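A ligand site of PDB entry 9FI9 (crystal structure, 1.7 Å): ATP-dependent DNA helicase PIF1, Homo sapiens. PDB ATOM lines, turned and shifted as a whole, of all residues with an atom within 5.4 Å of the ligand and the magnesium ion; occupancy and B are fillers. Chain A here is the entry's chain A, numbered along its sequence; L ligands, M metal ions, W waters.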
ATOM      1  N   MET A   3      10.547  36.011  -4.426  1.00  0.00           N
ATOM      2  CA  MET A   3      11.347  36.634  -3.387  1.00  0.00           C
ATOM      3  C   MET A   3      12.799  36.787  -3.853  1.00  0.00           C
ATOM      4  O   MET A   3      13.233  36.132  -4.795  1.00  0.00           O
ATOM      5  CB  MET A   3      11.283  35.861  -2.064  1.00  0.00           C
ATOM      6  CG  MET A   3       9.885  35.808  -1.484  1.00  0.00           C
ATOM      7  SD  MET A   3       9.789  35.083   0.174  1.00  0.00           S
ATOM      8  CE  MET A   3      10.285  33.422  -0.283  1.00  0.00           C
ATOM      9  N   GLN A   4      13.531  37.685  -3.184  1.00  0.00           N
ATOM     10  CA  GLN A   4      14.916  37.977  -3.521  1.00  0.00           C
ATOM     11  C   GLN A   4      15.804  36.977  -2.788  1.00  0.00           C
ATOM     12  O   GLN A   4      15.810  36.957  -1.552  1.00  0.00           O
ATOM     13  CB  GLN A   4      15.227  39.439  -3.157  1.00  0.00           C
ATOM     14  CG  GLN A   4      16.685  39.866  -3.309  1.00  0.00           C
ATOM     15  CD  GLN A   4      17.262  39.656  -4.699  1.00  0.00           C
ATOM     16  OE1 GLN A   4      18.274  38.972  -4.889  1.00  0.00           O
ATOM     17  NE2 GLN A   4      16.626  40.269  -5.679  1.00  0.00           N
ATOM     18  N   LEU A   5      16.547  36.144  -3.534  1.00  0.00           N
ATOM     19  CA  LEU A   5      17.426  35.159  -2.918  1.00  0.00           C
ATOM     20  C   LEU A   5      18.499  35.885  -2.119  1.00  0.00           C
ATOM     21  O   LEU A   5      18.972  36.934  -2.541  1.00  0.00           O
ATOM     22  CB  LEU A   5      18.059  34.259  -3.982  1.00  0.00           C
ATOM     23  CG  LEU A   5      17.138  33.312  -4.738  1.00  0.00           C
ATOM     24  CD1 LEU A   5      17.981  32.445  -5.687  1.00  0.00           C
ATOM     25  CD2 LEU A   5      16.235  32.444  -3.859  1.00  0.00           C
ATOM     26  N   SER A   6      18.843  35.364  -0.958  1.00  0.00           N
ATOM     27  CA  SER A   6      20.038  35.843  -0.283  1.00  0.00           C
ATOM     28  C   SER A   6      21.275  35.598  -1.156  1.00  0.00           C
ATOM     29  O   SER A   6      21.246  34.815  -2.125  1.00  0.00           O
ATOM     30  CB  SER A   6      20.175  35.165   1.057  1.00  0.00           C
ATOM     31  OG  SER A   6      20.540  33.789   0.901  1.00  0.00           O
ATOM     32  N   GLN A   9      22.015  31.992  -1.017  1.00  0.00           N
ATOM     33  CA  GLN A   9      21.109  31.224  -1.859  1.00  0.00           C
ATOM     34  C   GLN A   9      21.516  31.371  -3.329  1.00  0.00           C
ATOM     35  O   GLN A   9      21.527  30.386  -4.076  1.00  0.00           O
ATOM     36  CB  GLN A   9      19.646  31.575  -1.643  1.00  0.00           C
ATOM     37  CG  GLN A   9      19.120  31.157  -0.259  1.00  0.00           C
ATOM     38  CD  GLN A   9      17.688  31.616  -0.066  1.00  0.00           C
ATOM     39  OE1 GLN A   9      17.397  32.770  -0.413  1.00  0.00           O
ATOM     40  NE2 GLN A   9      16.776  30.742   0.357  1.00  0.00           N
ATOM     41  N   GLY A  26      22.160  23.638   6.083  1.00  0.00           N
ATOM     42  CA  GLY A  26      21.786  24.768   6.904  1.00  0.00           C
ATOM     43  C   GLY A  26      20.721  24.377   7.933  1.00  0.00           C
ATOM     44  O   GLY A  26      20.008  23.381   7.753  1.00  0.00           O
ATOM     45  N   SER A  27      20.603  25.189   8.996  1.00  0.00           N
ATOM     46  CA  SER A  27      19.579  24.977  10.024  1.00  0.00           C
ATOM     47  C   SER A  27      18.168  24.895   9.452  1.00  0.00           C
ATOM     48  O   SER A  27      17.873  25.283   8.332  1.00  0.00           O
ATOM     49  CB  SER A  27      19.638  26.155  11.072  1.00  0.00           C
ATOM     50  OG  SER A  27      20.953  26.111  11.618  1.00  0.00           O
ATOM     51  N   ALA A  28      17.261  24.395  10.277  1.00  0.00           N
ATOM     52  CA  ALA A  28      15.838  24.406   9.974  1.00  0.00           C
ATOM     53  C   ALA A  28      15.416  25.824   9.564  1.00  0.00           C
ATOM     54  O   ALA A  28      15.797  26.810  10.194  1.00  0.00           O
ATOM     55  CB  ALA A  28      15.082  23.914  11.194  1.00  0.00           C
ATOM     56  N   GLY A  29      14.656  25.913   8.453  1.00  0.00           N
ATOM     57  CA  GLY A  29      14.011  27.170   8.119  1.00  0.00           C
ATOM     58  C   GLY A  29      14.930  28.187   7.450  1.00  0.00           C
ATOM     59  O   GLY A  29      14.598  29.389   7.433  1.00  0.00           O
ATOM     60  N   THR A  30      16.024  27.724   6.880  1.00  0.00           N
ATOM     61  CA  THR A  30      17.017  28.550   6.181  1.00  0.00           C
ATOM     62  C   THR A  30      16.689  28.668   4.688  1.00  0.00           C
ATOM     63  O   THR A  30      17.436  29.298   3.932  1.00  0.00           O
ATOM     64  CB  THR A  30      18.465  28.106   6.452  1.00  0.00           C
ATOM     65  OG1 THR A  30      18.560  26.702   6.166  1.00  0.00           O
ATOM     66  CG2 THR A  30      18.976  28.457   7.845  1.00  0.00           C
ATOM     67  N   GLY A  31      15.577  28.059   4.236  1.00  0.00           N
ATOM     68  CA  GLY A  31      15.145  28.169   2.843  1.00  0.00           C
ATOM     69  C   GLY A  31      15.756  27.149   1.874  1.00  0.00           C
ATOM     70  O   GLY A  31      15.912  27.486   0.703  1.00  0.00           O
ATOM     71  N   LYS A  32      16.216  25.975   2.377  1.00  0.00           N
ATOM     72  CA  LYS A  32      16.832  24.941   1.558  1.00  0.00           C
ATOM     73  C   LYS A  32      15.808  24.422   0.536  1.00  0.00           C
ATOM     74  O   LYS A  32      16.063  24.402  -0.661  1.00  0.00           O
ATOM     75  CB  LYS A  32      17.273  23.760   2.440  1.00  0.00           C
ATOM     76  CG  LYS A  32      18.453  24.142   3.376  1.00  0.00           C
ATOM     77  CD  LYS A  32      18.998  22.966   4.203  1.00  0.00           C
ATOM     78  CE  LYS A  32      18.037  22.348   5.168  1.00  0.00           C
ATOM     79  NZ  LYS A  32      17.521  23.313   6.195  1.00  0.00           N
ATOM     80  N   SER A  33      14.634  24.027   1.015  1.00  0.00           N
ATOM     81  CA  SER A  33      13.622  23.485   0.107  1.00  0.00           C
ATOM     82  C   SER A  33      13.075  24.528  -0.870  1.00  0.00           C
ATOM     83  O   SER A  33      12.783  24.205  -2.028  1.00  0.00           O
ATOM     84  CB  SER A  33      12.477  22.821   0.880  1.00  0.00           C
ATOM     85  OG  SER A  33      12.997  21.764   1.685  1.00  0.00           O
ATOM     86  N   TYR A  34      12.902  25.762  -0.395  1.00  0.00           N
ATOM     87  CA  TYR A  34      12.504  26.877  -1.246  1.00  0.00           C
ATOM     88  C   TYR A  34      13.536  27.075  -2.358  1.00  0.00           C
ATOM     89  O   TYR A  34      13.174  27.310  -3.537  1.00  0.00           O
ATOM     90  CB  TYR A  34      12.398  28.132  -0.364  1.00  0.00           C
ATOM     91  CG  TYR A  34      12.148  29.362  -1.228  1.00  0.00           C
ATOM     92  CD1 TYR A  34      10.916  29.559  -1.837  1.00  0.00           C
ATOM     93  CD2 TYR A  34      13.171  30.265  -1.515  1.00  0.00           C
ATOM     94  CE1 TYR A  34      10.675  30.628  -2.690  1.00  0.00           C
ATOM     95  CE2 TYR A  34      12.932  31.350  -2.350  1.00  0.00           C
ATOM     96  CZ  TYR A  34      11.695  31.524  -2.924  1.00  0.00           C
ATOM     97  OH  TYR A  34      11.445  32.589  -3.736  1.00  0.00           O
ATOM     98  N   LEU A  35      14.824  27.002  -2.003  1.00  0.00           N
ATOM     99  CA  LEU A  35      15.872  27.180  -3.009  1.00  0.00           C
ATOM    100  C   LEU A  35      15.835  26.024  -4.015  1.00  0.00           C
ATOM    101  O   LEU A  35      16.076  26.215  -5.216  1.00  0.00           O
ATOM    102  CB  LEU A  35      17.221  27.264  -2.312  1.00  0.00           C
ATOM    103  CG  LEU A  35      18.386  27.622  -3.248  1.00  0.00           C
ATOM    104  CD1 LEU A  35      18.017  28.876  -4.053  1.00  0.00           C
ATOM    105  CD2 LEU A  35      19.687  27.799  -2.502  1.00  0.00           C
ATOM    106  N   ASP A 104      16.306  16.246  -1.658  1.00  0.00           N
ATOM    107  CA  ASP A 104      16.092  16.995  -0.419  1.00  0.00           C
ATOM    108  C   ASP A 104      16.082  16.001   0.758  1.00  0.00           C
ATOM    109  O   ASP A 104      15.879  14.789   0.571  1.00  0.00           O
ATOM    110  CB  ASP A 104      14.812  17.811  -0.528  1.00  0.00           C
ATOM    111  CG  ASP A 104      14.640  18.993   0.446  1.00  0.00           C
ATOM    112  OD1 ASP A 104      15.486  19.159   1.370  1.00  0.00           O
ATOM    113  OD2 ASP A 104      13.624  19.730   0.301  1.00  0.00           O
ATOM    114  N   GLU A 105      16.272  16.548   1.957  1.00  0.00           N
ATOM    115  CA  GLU A 105      16.270  15.838   3.217  1.00  0.00           C
ATOM    116  C   GLU A 105      17.241  14.644   3.202  1.00  0.00           C
ATOM    117  O   GLU A 105      16.881  13.522   3.579  1.00  0.00           O
ATOM    118  CB  GLU A 105      14.830  15.443   3.580  1.00  0.00           C
ATOM    119  CG  GLU A 105      13.970  16.674   3.911  1.00  0.00           C
ATOM    120  CD  GLU A 105      14.224  17.389   5.221  1.00  0.00           C
ATOM    121  OE1 GLU A 105      15.246  17.083   5.921  1.00  0.00           O
ATOM    122  OE2 GLU A 105      13.373  18.248   5.619  1.00  0.00           O
ATOM    123  N   ASP A 141      19.880  18.690   6.396  1.00  0.00           N
ATOM    124  CA  ASP A 141      20.594  19.063   7.601  1.00  0.00           C
ATOM    125  C   ASP A 141      20.863  17.787   8.384  1.00  0.00           C
ATOM    126  O   ASP A 141      19.932  17.168   8.901  1.00  0.00           O
ATOM    127  CB  ASP A 141      19.744  20.069   8.377  1.00  0.00           C
ATOM    128  CG  ASP A 141      20.314  20.524   9.711  1.00  0.00           C
ATOM    129  OD1 ASP A 141      21.447  20.114  10.033  1.00  0.00           O
ATOM    130  OD2 ASP A 141      19.641  21.328  10.385  1.00  0.00           O
ATOM    131  N   GLN A 144      19.266  17.340  11.698  1.00  0.00           N
ATOM    132  CA  GLN A 144      17.836  17.020  11.765  1.00  0.00           C
ATOM    133  C   GLN A 144      17.608  15.484  11.779  1.00  0.00           C
ATOM    134  O   GLN A 144      18.232  14.751  12.562  1.00  0.00           O
ATOM    135  CB  GLN A 144      17.100  17.852  10.707  1.00  0.00           C
ATOM    136  CG  GLN A 144      17.021  19.338  11.046  1.00  0.00           C
ATOM    137  CD  GLN A 144      16.105  20.100  10.109  1.00  0.00           C
ATOM    138  OE1 GLN A 144      14.928  19.785   9.933  1.00  0.00           O
ATOM    139  NE2 GLN A 144      16.638  21.135   9.497  1.00  0.00           N
ATOM    140  N   TRP A 178      14.749  32.013   8.272  1.00  0.00           N
ATOM    141  CA  TRP A 178      13.602  32.779   7.828  1.00  0.00           C
ATOM    142  C   TRP A 178      12.322  32.317   8.525  1.00  0.00           C
ATOM    143  O   TRP A 178      11.389  33.099   8.686  1.00  0.00           O
ATOM    144  CB  TRP A 178      13.409  32.616   6.322  1.00  0.00           C
ATOM    145  CG  TRP A 178      14.611  32.989   5.493  1.00  0.00           C
ATOM    146  CD1 TRP A 178      15.503  32.147   4.897  1.00  0.00           C
ATOM    147  CD2 TRP A 178      15.035  34.336   5.179  1.00  0.00           C
ATOM    148  NE1 TRP A 178      16.467  32.880   4.240  1.00  0.00           N
ATOM    149  CE2 TRP A 178      16.196  34.211   4.388  1.00  0.00           C
ATOM    150  CE3 TRP A 178      14.541  35.607   5.490  1.00  0.00           C
ATOM    151  CZ2 TRP A 178      16.875  35.337   3.907  1.00  0.00           C
ATOM    152  CZ3 TRP A 178      15.205  36.714   4.994  1.00  0.00           C
ATOM    153  CH2 TRP A 178      16.359  36.573   4.218  1.00  0.00           C
ATOM    154  N   ARG A 179      12.253  31.015   8.863  1.00  0.00           N
ATOM    155  CA  ARG A 179      11.002  30.437   9.372  1.00  0.00           C
ATOM    156  C   ARG A 179      10.526  31.200  10.621  1.00  0.00           C
ATOM    157  O   ARG A 179       9.346  31.579  10.737  1.00  0.00           O
ATOM    158  CB  ARG A 179      11.071  28.923   9.620  1.00  0.00           C
ATOM    159  CG  ARG A 179       9.793  28.379  10.272  1.00  0.00           C
ATOM    160  CD  ARG A 179       9.884  26.890  10.588  1.00  0.00           C
ATOM    161  NE  ARG A 179       9.868  26.134   9.341  1.00  0.00           N
ATOM    162  CZ  ARG A 179      10.645  25.091   9.010  1.00  0.00           C
ATOM    163  NH1 ARG A 179      11.519  24.553   9.888  1.00  0.00           N
ATOM    164  NH2 ARG A 179      10.524  24.597   7.783  1.00  0.00           N
ATOM    165  N   GLY A 357      10.243  19.107   7.411  1.00  0.00           N
ATOM    166  CA  GLY A 357      10.224  20.120   6.359  1.00  0.00           C
ATOM    167  C   GLY A 357       9.090  21.150   6.464  1.00  0.00           C
ATOM    168  O   GLY A 357       9.127  22.125   5.731  1.00  0.00           O
ATOM    169  N   MET A 358       8.135  20.992   7.393  1.00  0.00           N
ATOM    170  CA  MET A 358       6.950  21.843   7.497  1.00  0.00           C
ATOM    171  C   MET A 358       7.135  23.010   8.449  1.00  0.00           C
ATOM    172  O   MET A 358       7.989  22.975   9.343  1.00  0.00           O
ATOM    173  CB  MET A 358       5.744  21.075   8.058  1.00  0.00           C
ATOM    174  CG  MET A 358       5.244  20.025   7.061  1.00  0.00           C
ATOM    175  SD  MET A 358       3.706  19.263   7.618  1.00  0.00           S
ATOM    176  CE  MET A 358       2.531  20.624   7.496  1.00  0.00           C
ATOM    177  N   THR A 359       6.305  24.067   8.275  1.00  0.00           N
ATOM    178  CA  THR A 359       6.138  25.109   9.290  1.00  0.00           C
ATOM    179  C   THR A 359       4.799  24.860   9.985  1.00  0.00           C
ATOM    180  O   THR A 359       3.825  24.626   9.302  1.00  0.00           O
ATOM    181  CB  THR A 359       6.174  26.499   8.653  1.00  0.00           C
ATOM    182  OG1 THR A 359       7.425  26.681   7.982  1.00  0.00           O
ATOM    183  CG2 THR A 359       5.916  27.570   9.694  1.00  0.00           C
ATOM    184  N   ARG A 382       9.803  23.402  14.112  1.00  0.00           N
ATOM    185  CA  ARG A 382       8.670  23.555  13.191  1.00  0.00           C
ATOM    186  C   ARG A 382       7.876  24.852  13.451  1.00  0.00           C
ATOM    187  O   ARG A 382       7.265  25.396  12.537  1.00  0.00           O
ATOM    188  CB  ARG A 382       7.681  22.408  13.396  1.00  0.00           C
ATOM    189  CG  ARG A 382       8.194  21.005  13.076  1.00  0.00           C
ATOM    190  CD  ARG A 382       8.882  20.807  11.709  1.00  0.00           C
ATOM    191  NE  ARG A 382      10.290  21.209  11.841  1.00  0.00           N
ATOM    192  CZ  ARG A 382      11.170  21.335  10.839  1.00  0.00           C
ATOM    193  NH1 ARG A 382      12.452  21.534  11.101  1.00  0.00           N
ATOM    194  NH2 ARG A 382      10.766  21.269   9.578  1.00  0.00           N
HETATM  195  P1  LIG L   1      13.677  22.577   6.974  1.00  0.00           P
HETATM  196  O1  LIG L   1      12.725  22.489   8.121  1.00  0.00           O
HETATM  197  O2  LIG L   1      13.240  21.619   5.891  1.00  0.00           O
HETATM  198  O3  LIG L   1      15.144  22.390   7.287  1.00  0.00           O
HETATM  199  P2  LIG L   1      14.195  24.641   4.963  1.00  0.00           P
HETATM  200  O4  LIG L   1      13.886  23.786   3.794  1.00  0.00           O
HETATM  201  O5  LIG L   1      15.631  25.088   5.104  1.00  0.00           O
HETATM  202  N1  LIG L   1      13.449  24.106   6.324  1.00  0.00           N
HETATM  203  P3  LIG L   1      12.065  26.240   3.755  1.00  0.00           P
HETATM  204  O6  LIG L   1      11.013  25.393   4.418  1.00  0.00           O
HETATM  205  O7  LIG L   1      12.398  26.055   2.317  1.00  0.00           O
HETATM  206  O8  LIG L   1      13.380  25.981   4.675  1.00  0.00           O
HETATM  207  O9  LIG L   1      11.806  27.810   4.029  1.00  0.00           O
HETATM  208  C1  LIG L   1      11.398  28.308   5.310  1.00  0.00           C
HETATM  209  C2  LIG L   1      10.762  29.659   5.090  1.00  0.00           C
HETATM  210  O10 LIG L   1      11.748  30.611   4.627  1.00  0.00           O
HETATM  211  C3  LIG L   1       9.664  29.655   4.014  1.00  0.00           C
HETATM  212  O11 LIG L   1       8.521  30.326   4.539  1.00  0.00           O
HETATM  213  C4  LIG L   1      10.286  30.414   2.849  1.00  0.00           C
HETATM  214  O12 LIG L   1       9.375  31.229   2.148  1.00  0.00           O
HETATM  215  C5  LIG L   1      11.213  31.384   3.570  1.00  0.00           C
HETATM  216  N2  LIG L   1      12.288  31.889   2.722  1.00  0.00           N
HETATM  217  C6  LIG L   1      13.217  31.132   1.977  1.00  0.00           C
HETATM  218  N3  LIG L   1      14.094  31.890   1.360  1.00  0.00           N
HETATM  219  C7  LIG L   1      13.707  33.196   1.655  1.00  0.00           C
HETATM  220  C8  LIG L   1      14.225  34.456   1.268  1.00  0.00           C
HETATM  221  N4  LIG L   1      15.238  34.608   0.424  1.00  0.00           N
HETATM  222  N5  LIG L   1      13.620  35.562   1.766  1.00  0.00           N
HETATM  223  C9  LIG L   1      12.580  35.409   2.597  1.00  0.00           C
HETATM  224  N6  LIG L   1      12.006  34.287   3.024  1.00  0.00           N
HETATM  225  C10 LIG L   1      12.612  33.200   2.499  1.00  0.00           C
HETATM  226 MG    MG M   1      13.093  21.767   3.871  1.00  0.00          MG
HETATM  227  O   HOH W   1      14.154  38.086   1.060  1.00  0.00           O
HETATM  228  O   HOH W   2      12.247  19.724   3.759  1.00  0.00           O
HETATM  229  O   HOH W   3      10.194  34.925   5.115  1.00  0.00           O
HETATM  230  O   HOH W   4       9.562  25.862   0.953  1.00  0.00           O
HETATM  231  O   HOH W   5       7.984  30.159   0.312  1.00  0.00           O
HETATM  232  O   HOH W   6      16.150  19.985   6.078  1.00  0.00           O
HETATM  233  O   HOH W   7       8.074  29.183   7.110  1.00  0.00           O
HETATM  234  O   HOH W   8       8.795  25.462   5.728  1.00  0.00           O
HETATM  235  O   HOH W   9       8.983  32.709   6.411  1.00  0.00           O
HETATM  236  O   HOH W  10      15.069  20.820   3.614  1.00  0.00           O
HETATM  237  O   HOH W  11      11.188  22.635   3.918  1.00  0.00           O
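OG of Ser 33 sits close to OD2 of Asp 104 (2.5 Å). N of Arg 179 is in hydrogen-bond range of O of Gly 29, at 3.2 Å. The backbone NH of Gln 9 is in hydrogen-bond range of the side-chain hydroxyl of Ser 6 (3.0 Å). The side-chain amide oxygen of Gln 144 is in hydrogen-bond range of the guanidinium group of Arg 382 (3.2 Å). NE2 of Gln 144 sits close to N of Ala 28, 3.4 Å away. N of Trp 178 is in hydrogen-bond range of O of Gly 29 (2.8 Å). NE2 of Gln 9 lies within hydrogen-bond range of O of Gly 31, at 3.4 Å. NZ of Lys 32 is in hydrogen-bond range of O of Ser 27, 2.9 Å away.
The magnesium ion is bound by an oxygen (O2) of the ligand. Water W11 is bound to the magnesium ion (2.1 Å). O4 of the ligand is bound to the magnesium ion (2.2 Å). OG of Ser 33 is bound to the magnesium ion. Water W10 is bound to the magnesium ion (2.2 Å). Water W2 binds the magnesium ion, at 2.2 Å.
The side-chain sulfur (SD) of Met 3 lies close to a nitrogen (N6) of the ligand. N of Gly 29 sits close to N1 of the ligand (3.0 Å). An oxygen (O2) of the ligand sits close to the side-chain carboxylate of Glu 105. N of Ser 6 touches N4 of the ligand, at 3.9 Å. O of Ser 27 touches O5 of the ligand (3.9 Å). Ala 28 touches the ligand (CA to O3, 3.4 Å). Trp 178 touches the ligand (CB to O10, 3.1 Å). CA of Gly 357 touches O2 of the ligand (3.4 Å). Hydrophobic or aromatic side chains within 4 Å of the ligand: Met 3, Tyr 34 and Trp 178. Of the 25 residues printed, 18 come within 4 Å of the ligand. The nearest printed residue that does not touch the ligand is Leu 5 (4.03 Å).
OE2 of Glu 105 touches the magnesium ion (3.9 Å). Two residues have an atom within 4 Å of the magnesium ion: Ser 33 and Glu 105.
Water W11 lies within hydrogen-bond range of O of Gly 357 (2.8 Å) and O6 of the ligand (2.8 Å). Water W8 lies within hydrogen-bond range of O6 of the ligand (2.6 Å), NH2 of Arg 179 (2.8 Å), OG1 of Thr 359 (2.9 Å) and O of Gly 357 (3.4 Å). Water W1 lies within hydrogen-bond range of N5 of the ligand and O of Gln 4. Water W7 bridges the side-chain hydroxyl of Thr 359 (2.7 Å) and an oxygen (O11) of the ligand (2.8 Å). Water W6 bridges an oxygen (O3) of the ligand (2.9 Å) and the side-chain carboxylate of Glu 105 (3.0 Å). Water W9 lies within hydrogen-bond range of O11 of the ligand (3.1 Å) and O of Trp 178 (3.3 Å).
The backbone NH (N) of Tyr 34 sits at hydrogen-bond distance from an oxygen (O7) of the ligand (2.8 Å). An oxygen (O1) of the ligand lies within salt-bridge range of the guanidinium group (NH1) of Arg 179 (3.0 Å). The backbone carbonyl oxygen (O) of Gln 4 sits at hydrogen-bond distance from a nitrogen (N4) of the ligand (3.1 Å). The side-chain amide oxygen (OE1) of Gln 9 sits at hydrogen-bond distance from a nitrogen (N4) of the ligand, 3.0 Å away. The backbone NH (N) of Thr 30 is in hydrogen-bond range of an oxygen (O5) of the ligand. The backbone NH of Lys 32 is in hydrogen-bond range of an oxygen (O5) of the ligand (2.9 Å). The backbone NH (N) of Gly 31 sits at hydrogen-bond distance from an oxygen (O8) of the ligand (3.1 Å). The side-chain amino group (NZ) of Lys 32 is in salt-bridge range of an oxygen (O3) of the ligand (2.8 Å). N of Ser 33 lies within hydrogen-bond range of O7 of the ligand. The side-chain amide nitrogen (NE2) of Gln 144 sits at hydrogen-bond distance from an oxygen (O3) of the ligand (2.9 Å). An oxygen (O1) of the ligand is in salt-bridge range of the guanidinium group (NH2) of Arg 382 (2.7 Å).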
